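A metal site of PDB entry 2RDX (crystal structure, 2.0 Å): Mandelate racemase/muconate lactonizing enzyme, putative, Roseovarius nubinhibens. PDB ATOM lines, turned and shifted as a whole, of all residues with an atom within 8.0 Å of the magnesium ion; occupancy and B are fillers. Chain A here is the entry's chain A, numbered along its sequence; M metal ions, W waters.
Asn 197 touches the magnesium ion.
Glu 244 touches the magnesium ion.
Within 4 Å of the magnesium ion: Asp 195, Asn 197, Glu 220, Asp 243 and Glu 244.
The nearest printed residue that does not touch the magnesium ion is Lys 267 (4.2 Å).
Water W1 bridges OH of Tyr 59 (2.5 Å) and ND2 of Asn 197 (2.9 Å).
Water W2 lies within hydrogen-bond range of the side-chain carboxylate of Asp 195 (2.6 Å), the side-chain carboxylate of Glu 244 (2.6 Å) and the side-chain amide nitrogen of Asn 197 (3.2 Å).
The side-chain amino group (NZ) of Lys 267 is in salt-bridge range of the side-chain carboxylate (OD1) of Asp 243 (3.2 Å).
The side-chain carboxylate of Asp 243 lies close to the side-chain sulfur of Cys 265 (3.6 Å).
The backbone NH (N) of Asp 243 sits at hydrogen-bond distance from the side-chain amide oxygen (OE1) of Gln 221 (2.7 Å).
The backbone carbonyl oxygen of Glu 220 lies within hydrogen-bond range of the backbone NH of Ala 196, at 3.2 Å.
The backbone carbonyl oxygen of Ala 194 lies within hydrogen-bond range of the backbone NH of Glu 220 (2.8 Å).
The side-chain carboxylate of Asp 195 sits at hydrogen-bond distance from the backbone NH of Asn 197, 2.9 Å away.
The side-chain carboxylate of Asp 195 lies close to the side-chain amide nitrogen of Gln 165, at 3.3 Å.
The backbone NH (N) of Glu 244 lies within hydrogen-bond range of the side-chain amide oxygen (OE1) of Gln 221.
Water W1 binds the magnesium ion (1.9 Å).
OD2 of Asp 243 is bound to the magnesium ion.
OE2 of Glu 220 binds the magnesium ion, 2.2 Å away.
Water W2 binds the magnesium ion (2.2 Å).
Water W3 is bound to the magnesium ion, 2.3 Å away.
OD2 of Asp 195 is bound to the magnesium ion, at 2.3 Å.
The magnesium ion has six donor atoms within binding distance.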
ATOM      1  N   TYR A  22     -13.306 -29.556  19.028  1.00  0.00           N
ATOM      2  CA  TYR A  22     -11.924 -29.136  19.317  1.00  0.00           C
ATOM      3  C   TYR A  22     -10.934 -30.011  18.545  1.00  0.00           C
ATOM      4  O   TYR A  22     -10.696 -31.170  18.910  1.00  0.00           O
ATOM      5  CB  TYR A  22     -11.646 -29.199  20.833  1.00  0.00           C
ATOM      6  CG  TYR A  22     -10.311 -28.626  21.274  1.00  0.00           C
ATOM      7  CD1 TYR A  22      -9.208 -29.449  21.502  1.00  0.00           C
ATOM      8  CD2 TYR A  22     -10.159 -27.255  21.493  1.00  0.00           C
ATOM      9  CE1 TYR A  22      -7.988 -28.932  21.919  1.00  0.00           C
ATOM     10  CE2 TYR A  22      -8.942 -26.714  21.905  1.00  0.00           C
ATOM     11  CZ  TYR A  22      -7.859 -27.558  22.121  1.00  0.00           C
ATOM     12  OH  TYR A  22      -6.650 -27.040  22.530  1.00  0.00           O
ATOM     13  N   TYR A  59      -5.243 -39.068  24.116  1.00  0.00           N
ATOM     14  CA  TYR A  59      -4.314 -37.946  24.205  1.00  0.00           C
ATOM     15  C   TYR A  59      -2.999 -38.301  24.915  1.00  0.00           C
ATOM     16  O   TYR A  59      -1.904 -37.986  24.438  1.00  0.00           O
ATOM     17  CB  TYR A  59      -5.037 -36.809  24.921  1.00  0.00           C
ATOM     18  CG  TYR A  59      -4.310 -35.480  24.943  1.00  0.00           C
ATOM     19  CD1 TYR A  59      -4.513 -34.541  23.951  1.00  0.00           C
ATOM     20  CD2 TYR A  59      -3.450 -35.162  25.990  1.00  0.00           C
ATOM     21  CE1 TYR A  59      -3.864 -33.321  23.986  1.00  0.00           C
ATOM     22  CE2 TYR A  59      -2.793 -33.954  26.025  1.00  0.00           C
ATOM     23  CZ  TYR A  59      -2.992 -33.037  25.024  1.00  0.00           C
ATOM     24  OH  TYR A  59      -2.324 -31.838  25.089  1.00  0.00           O
ATOM     25  N   TYR A 138      -2.653 -18.030  27.483  1.00  0.00           N
ATOM     26  CA  TYR A 138      -2.631 -17.985  26.018  1.00  0.00           C
ATOM     27  C   TYR A 138      -4.062 -18.083  25.453  1.00  0.00           C
ATOM     28  O   TYR A 138      -4.963 -18.594  26.112  1.00  0.00           O
ATOM     29  CB  TYR A 138      -1.728 -19.101  25.467  1.00  0.00           C
ATOM     30  CG  TYR A 138      -2.264 -20.493  25.698  1.00  0.00           C
ATOM     31  CD1 TYR A 138      -3.082 -21.121  24.755  1.00  0.00           C
ATOM     32  CD2 TYR A 138      -1.961 -21.194  26.866  1.00  0.00           C
ATOM     33  CE1 TYR A 138      -3.592 -22.395  24.959  1.00  0.00           C
ATOM     34  CE2 TYR A 138      -2.463 -22.480  27.070  1.00  0.00           C
ATOM     35  CZ  TYR A 138      -3.267 -23.073  26.126  1.00  0.00           C
ATOM     36  OH  TYR A 138      -3.749 -24.338  26.341  1.00  0.00           O
ATOM     37  N   GLN A 165      -1.680 -19.840  20.685  1.00  0.00           N
ATOM     38  CA  GLN A 165      -1.448 -21.208  20.244  1.00  0.00           C
ATOM     39  C   GLN A 165      -1.963 -21.448  18.819  1.00  0.00           C
ATOM     40  O   GLN A 165      -3.157 -21.362  18.567  1.00  0.00           O
ATOM     41  CB  GLN A 165      -2.106 -22.186  21.209  1.00  0.00           C
ATOM     42  CG  GLN A 165      -1.503 -23.571  21.168  1.00  0.00           C
ATOM     43  CD  GLN A 165      -2.361 -24.583  21.877  1.00  0.00           C
ATOM     44  OE1 GLN A 165      -3.569 -24.683  21.626  1.00  0.00           O
ATOM     45  NE2 GLN A 165      -1.749 -25.354  22.769  1.00  0.00           N
ATOM     46  N   MET A 193       2.974 -20.304  19.764  1.00  0.00           N
ATOM     47  CA  MET A 193       3.367 -21.698  19.941  1.00  0.00           C
ATOM     48  C   MET A 193       2.634 -22.624  18.981  1.00  0.00           C
ATOM     49  O   MET A 193       1.406 -22.704  18.988  1.00  0.00           O
ATOM     50  CB  MET A 193       3.249 -22.157  21.393  1.00  0.00           C
ATOM     51  CG  MET A 193       2.020 -21.711  22.136  1.00  0.00           C
ATOM     52  SD  MET A 193       2.507 -21.306  23.818  1.00  0.00           S
ATOM     53  CE  MET A 193       2.939 -19.595  23.575  1.00  0.00           C
ATOM     54  N   ALA A 194       3.403 -23.296  18.132  1.00  0.00           N
ATOM     55  CA  ALA A 194       2.859 -24.234  17.171  1.00  0.00           C
ATOM     56  C   ALA A 194       2.803 -25.599  17.830  1.00  0.00           C
ATOM     57  O   ALA A 194       3.818 -26.285  17.950  1.00  0.00           O
ATOM     58  CB  ALA A 194       3.712 -24.272  15.902  1.00  0.00           C
ATOM     59  N   ASP A 195       1.616 -25.964  18.266  1.00  0.00           N
ATOM     60  CA  ASP A 195       1.415 -27.253  18.925  1.00  0.00           C
ATOM     61  C   ASP A 195       0.923 -28.276  17.920  1.00  0.00           C
ATOM     62  O   ASP A 195      -0.199 -28.160  17.409  1.00  0.00           O
ATOM     63  CB  ASP A 195       0.418 -27.122  20.081  1.00  0.00           C
ATOM     64  CG  ASP A 195       0.533 -28.253  21.098  1.00  0.00           C
ATOM     65  OD1 ASP A 195       1.108 -29.310  20.777  1.00  0.00           O
ATOM     66  OD2 ASP A 195       0.070 -28.083  22.238  1.00  0.00           O
ATOM     67  N   ALA A 196       1.774 -29.267  17.626  1.00  0.00           N
ATOM     68  CA  ALA A 196       1.389 -30.365  16.738  1.00  0.00           C
ATOM     69  C   ALA A 196       0.653 -31.450  17.487  1.00  0.00           C
ATOM     70  O   ALA A 196       0.002 -32.300  16.871  1.00  0.00           O
ATOM     71  CB  ALA A 196       2.602 -30.938  16.052  1.00  0.00           C
ATOM     72  N   ASN A 197       0.790 -31.435  18.817  1.00  0.00           N
ATOM     73  CA  ASN A 197       0.111 -32.376  19.711  1.00  0.00           C
ATOM     74  C   ASN A 197       0.384 -33.828  19.333  1.00  0.00           C
ATOM     75  O   ASN A 197      -0.544 -34.613  19.134  1.00  0.00           O
ATOM     76  CB  ASN A 197      -1.401 -32.092  19.791  1.00  0.00           C
ATOM     77  CG  ASN A 197      -1.721 -30.840  20.587  1.00  0.00           C
ATOM     78  OD1 ASN A 197      -2.386 -29.928  20.082  1.00  0.00           O
ATOM     79  ND2 ASN A 197      -1.237 -30.787  21.816  1.00  0.00           N
ATOM     80  N   GLN A 198       1.680 -34.149  19.246  1.00  0.00           N
ATOM     81  CA  GLN A 198       2.191 -35.474  18.838  1.00  0.00           C
ATOM     82  C   GLN A 198       1.857 -35.858  17.389  1.00  0.00           C
ATOM     83  O   GLN A 198       1.960 -37.024  17.007  1.00  0.00           O
ATOM     84  CB  GLN A 198       1.717 -36.570  19.805  1.00  0.00           C
ATOM     85  CG  GLN A 198       1.972 -36.262  21.283  1.00  0.00           C
ATOM     86  CD  GLN A 198       1.428 -37.325  22.193  1.00  0.00           C
ATOM     87  OE1 GLN A 198       2.152 -37.873  23.024  1.00  0.00           O
ATOM     88  NE2 GLN A 198       0.151 -37.637  22.054  1.00  0.00           N
ATOM     89  N   GLU A 220       6.151 -26.823  19.451  1.00  0.00           N
ATOM     90  CA  GLU A 220       5.628 -27.598  20.587  1.00  0.00           C
ATOM     91  C   GLU A 220       5.239 -29.062  20.287  1.00  0.00           C
ATOM     92  O   GLU A 220       4.420 -29.329  19.402  1.00  0.00           O
ATOM     93  CB  GLU A 220       4.468 -26.857  21.255  1.00  0.00           C
ATOM     94  CG  GLU A 220       3.843 -27.646  22.402  1.00  0.00           C
ATOM     95  CD  GLU A 220       2.812 -26.864  23.187  1.00  0.00           C
ATOM     96  OE1 GLU A 220       2.553 -25.686  22.865  1.00  0.00           O
ATOM     97  OE2 GLU A 220       2.257 -27.466  24.128  1.00  0.00           O
ATOM     98  N   GLN A 221       5.799 -29.983  21.084  1.00  0.00           N
ATOM     99  CA  GLN A 221       5.574 -31.443  20.966  1.00  0.00           C
ATOM    100  C   GLN A 221       5.343 -31.929  19.509  1.00  0.00           C
ATOM    101  O   GLN A 221       4.277 -32.482  19.212  1.00  0.00           O
ATOM    102  CB  GLN A 221       4.434 -31.865  21.908  1.00  0.00           C
ATOM    103  CG  GLN A 221       4.271 -33.371  22.141  1.00  0.00           C
ATOM    104  CD  GLN A 221       5.316 -33.990  23.035  1.00  0.00           C
ATOM    105  OE1 GLN A 221       5.747 -33.392  24.016  1.00  0.00           O
ATOM    106  NE2 GLN A 221       5.725 -35.221  22.714  1.00  0.00           N
ATOM    107  N   LYS A 241       9.128 -26.908  23.050  1.00  0.00           N
ATOM    108  CA  LYS A 241       8.307 -27.168  24.207  1.00  0.00           C
ATOM    109  C   LYS A 241       7.892 -28.633  24.205  1.00  0.00           C
ATOM    110  O   LYS A 241       7.331 -29.122  23.222  1.00  0.00           O
ATOM    111  CB  LYS A 241       7.090 -26.243  24.209  1.00  0.00           C
ATOM    112  CG  LYS A 241       6.208 -26.425  25.423  1.00  0.00           C
ATOM    113  CD  LYS A 241       5.130 -25.369  25.509  1.00  0.00           C
ATOM    114  CE  LYS A 241       4.036 -25.870  26.414  1.00  0.00           C
ATOM    115  NZ  LYS A 241       2.784 -25.074  26.289  1.00  0.00           N
ATOM    116  N   LEU A 242       8.198 -29.348  25.286  1.00  0.00           N
ATOM    117  CA  LEU A 242       7.739 -30.716  25.423  1.00  0.00           C
ATOM    118  C   LEU A 242       6.551 -30.740  26.361  1.00  0.00           C
ATOM    119  O   LEU A 242       6.491 -29.994  27.333  1.00  0.00           O
ATOM    120  CB  LEU A 242       8.865 -31.643  25.903  1.00  0.00           C
ATOM    121  CG  LEU A 242      10.105 -31.805  24.997  1.00  0.00           C
ATOM    122  CD1 LEU A 242      11.208 -32.554  25.728  1.00  0.00           C
ATOM    123  CD2 LEU A 242       9.774 -32.506  23.690  1.00  0.00           C
ATOM    124  N   ASP A 243       5.606 -31.628  26.099  1.00  0.00           N
ATOM    125  CA  ASP A 243       4.337 -31.594  26.794  1.00  0.00           C
ATOM    126  C   ASP A 243       3.939 -32.999  27.202  1.00  0.00           C
ATOM    127  O   ASP A 243       4.246 -33.420  28.306  1.00  0.00           O
ATOM    128  CB  ASP A 243       3.281 -30.905  25.912  1.00  0.00           C
ATOM    129  CG  ASP A 243       1.947 -30.678  26.617  1.00  0.00           C
ATOM    130  OD1 ASP A 243       1.669 -31.329  27.644  1.00  0.00           O
ATOM    131  OD2 ASP A 243       1.156 -29.855  26.120  1.00  0.00           O
ATOM    132  N   GLU A 244       3.287 -33.730  26.296  1.00  0.00           N
ATOM    133  CA  GLU A 244       2.671 -35.014  26.633  1.00  0.00           C
ATOM    134  C   GLU A 244       3.638 -36.126  26.999  1.00  0.00           C
ATOM    135  O   GLU A 244       3.253 -37.105  27.653  1.00  0.00           O
ATOM    136  CB  GLU A 244       1.762 -35.473  25.500  1.00  0.00           C
ATOM    137  CG  GLU A 244       0.561 -34.561  25.295  1.00  0.00           C
ATOM    138  CD  GLU A 244       0.695 -33.707  24.057  1.00  0.00           C
ATOM    139  OE1 GLU A 244       1.420 -32.707  24.110  1.00  0.00           O
ATOM    140  OE2 GLU A 244       0.058 -34.026  23.037  1.00  0.00           O
ATOM    141  N   CYS A 265       6.075 -28.532  29.624  1.00  0.00           N
ATOM    142  CA  CYS A 265       4.658 -28.364  29.944  1.00  0.00           C
ATOM    143  C   CYS A 265       4.208 -29.377  30.995  1.00  0.00           C
ATOM    144  O   CYS A 265       4.343 -30.583  30.807  1.00  0.00           O
ATOM    145  CB  CYS A 265       3.802 -28.503  28.678  1.00  0.00           C
ATOM    146  SG  CYS A 265       2.079 -28.010  28.897  1.00  0.00           S
ATOM    147  N   LYS A 267       1.310 -30.959  32.946  1.00  0.00           N
ATOM    148  CA  LYS A 267      -0.097 -31.279  33.153  1.00  0.00           C
ATOM    149  C   LYS A 267      -0.253 -32.122  34.410  1.00  0.00           C
ATOM    150  O   LYS A 267       0.229 -33.258  34.469  1.00  0.00           O
ATOM    151  CB  LYS A 267      -0.657 -31.993  31.939  1.00  0.00           C
ATOM    152  CG  LYS A 267      -0.804 -31.117  30.704  1.00  0.00           C
ATOM    153  CD  LYS A 267      -1.811 -31.747  29.747  1.00  0.00           C
ATOM    154  CE  LYS A 267      -1.493 -31.488  28.298  1.00  0.00           C
ATOM    155  NZ  LYS A 267      -1.299 -30.055  27.969  1.00  0.00           N
ATOM    156  N   VAL A 292       5.261 -24.614  31.981  1.00  0.00           N
ATOM    157  CA  VAL A 292       3.842 -24.279  31.871  1.00  0.00           C
ATOM    158  C   VAL A 292       3.116 -25.090  32.937  1.00  0.00           C
ATOM    159  O   VAL A 292       3.456 -26.258  33.136  1.00  0.00           O
ATOM    160  CB  VAL A 292       3.292 -24.624  30.473  1.00  0.00           C
ATOM    161  CG1 VAL A 292       1.784 -24.521  30.449  1.00  0.00           C
ATOM    162  CG2 VAL A 292       3.891 -23.700  29.436  1.00  0.00           C
ATOM    163  N   GLU A 294      -0.448 -26.582  33.969  1.00  0.00           N
ATOM    164  CA  GLU A 294      -1.734 -26.906  33.346  1.00  0.00           C
ATOM    165  C   GLU A 294      -2.326 -28.200  33.880  1.00  0.00           C
ATOM    166  O   GLU A 294      -1.900 -28.755  34.881  1.00  0.00           O
ATOM    167  CB  GLU A 294      -1.532 -27.132  31.852  1.00  0.00           C
ATOM    168  CG  GLU A 294      -1.615 -25.930  30.976  1.00  0.00           C
ATOM    169  CD  GLU A 294      -1.496 -26.302  29.519  1.00  0.00           C
ATOM    170  OE1 GLU A 294      -1.048 -27.433  29.221  1.00  0.00           O
ATOM    171  OE2 GLU A 294      -1.861 -25.475  28.655  1.00  0.00           O
HETATM  172 MG    MG M   1       0.552 -28.816  24.400  1.00  0.00          MG
HETATM  173  O   HOH W   1      -1.079 -29.765  24.481  1.00  0.00           O
HETATM  174  O   HOH W   2       1.606 -30.286  23.133  1.00  0.00           O
HETATM  175  O   HOH W   3      -0.363 -26.768  25.043  1.00  0.00           O
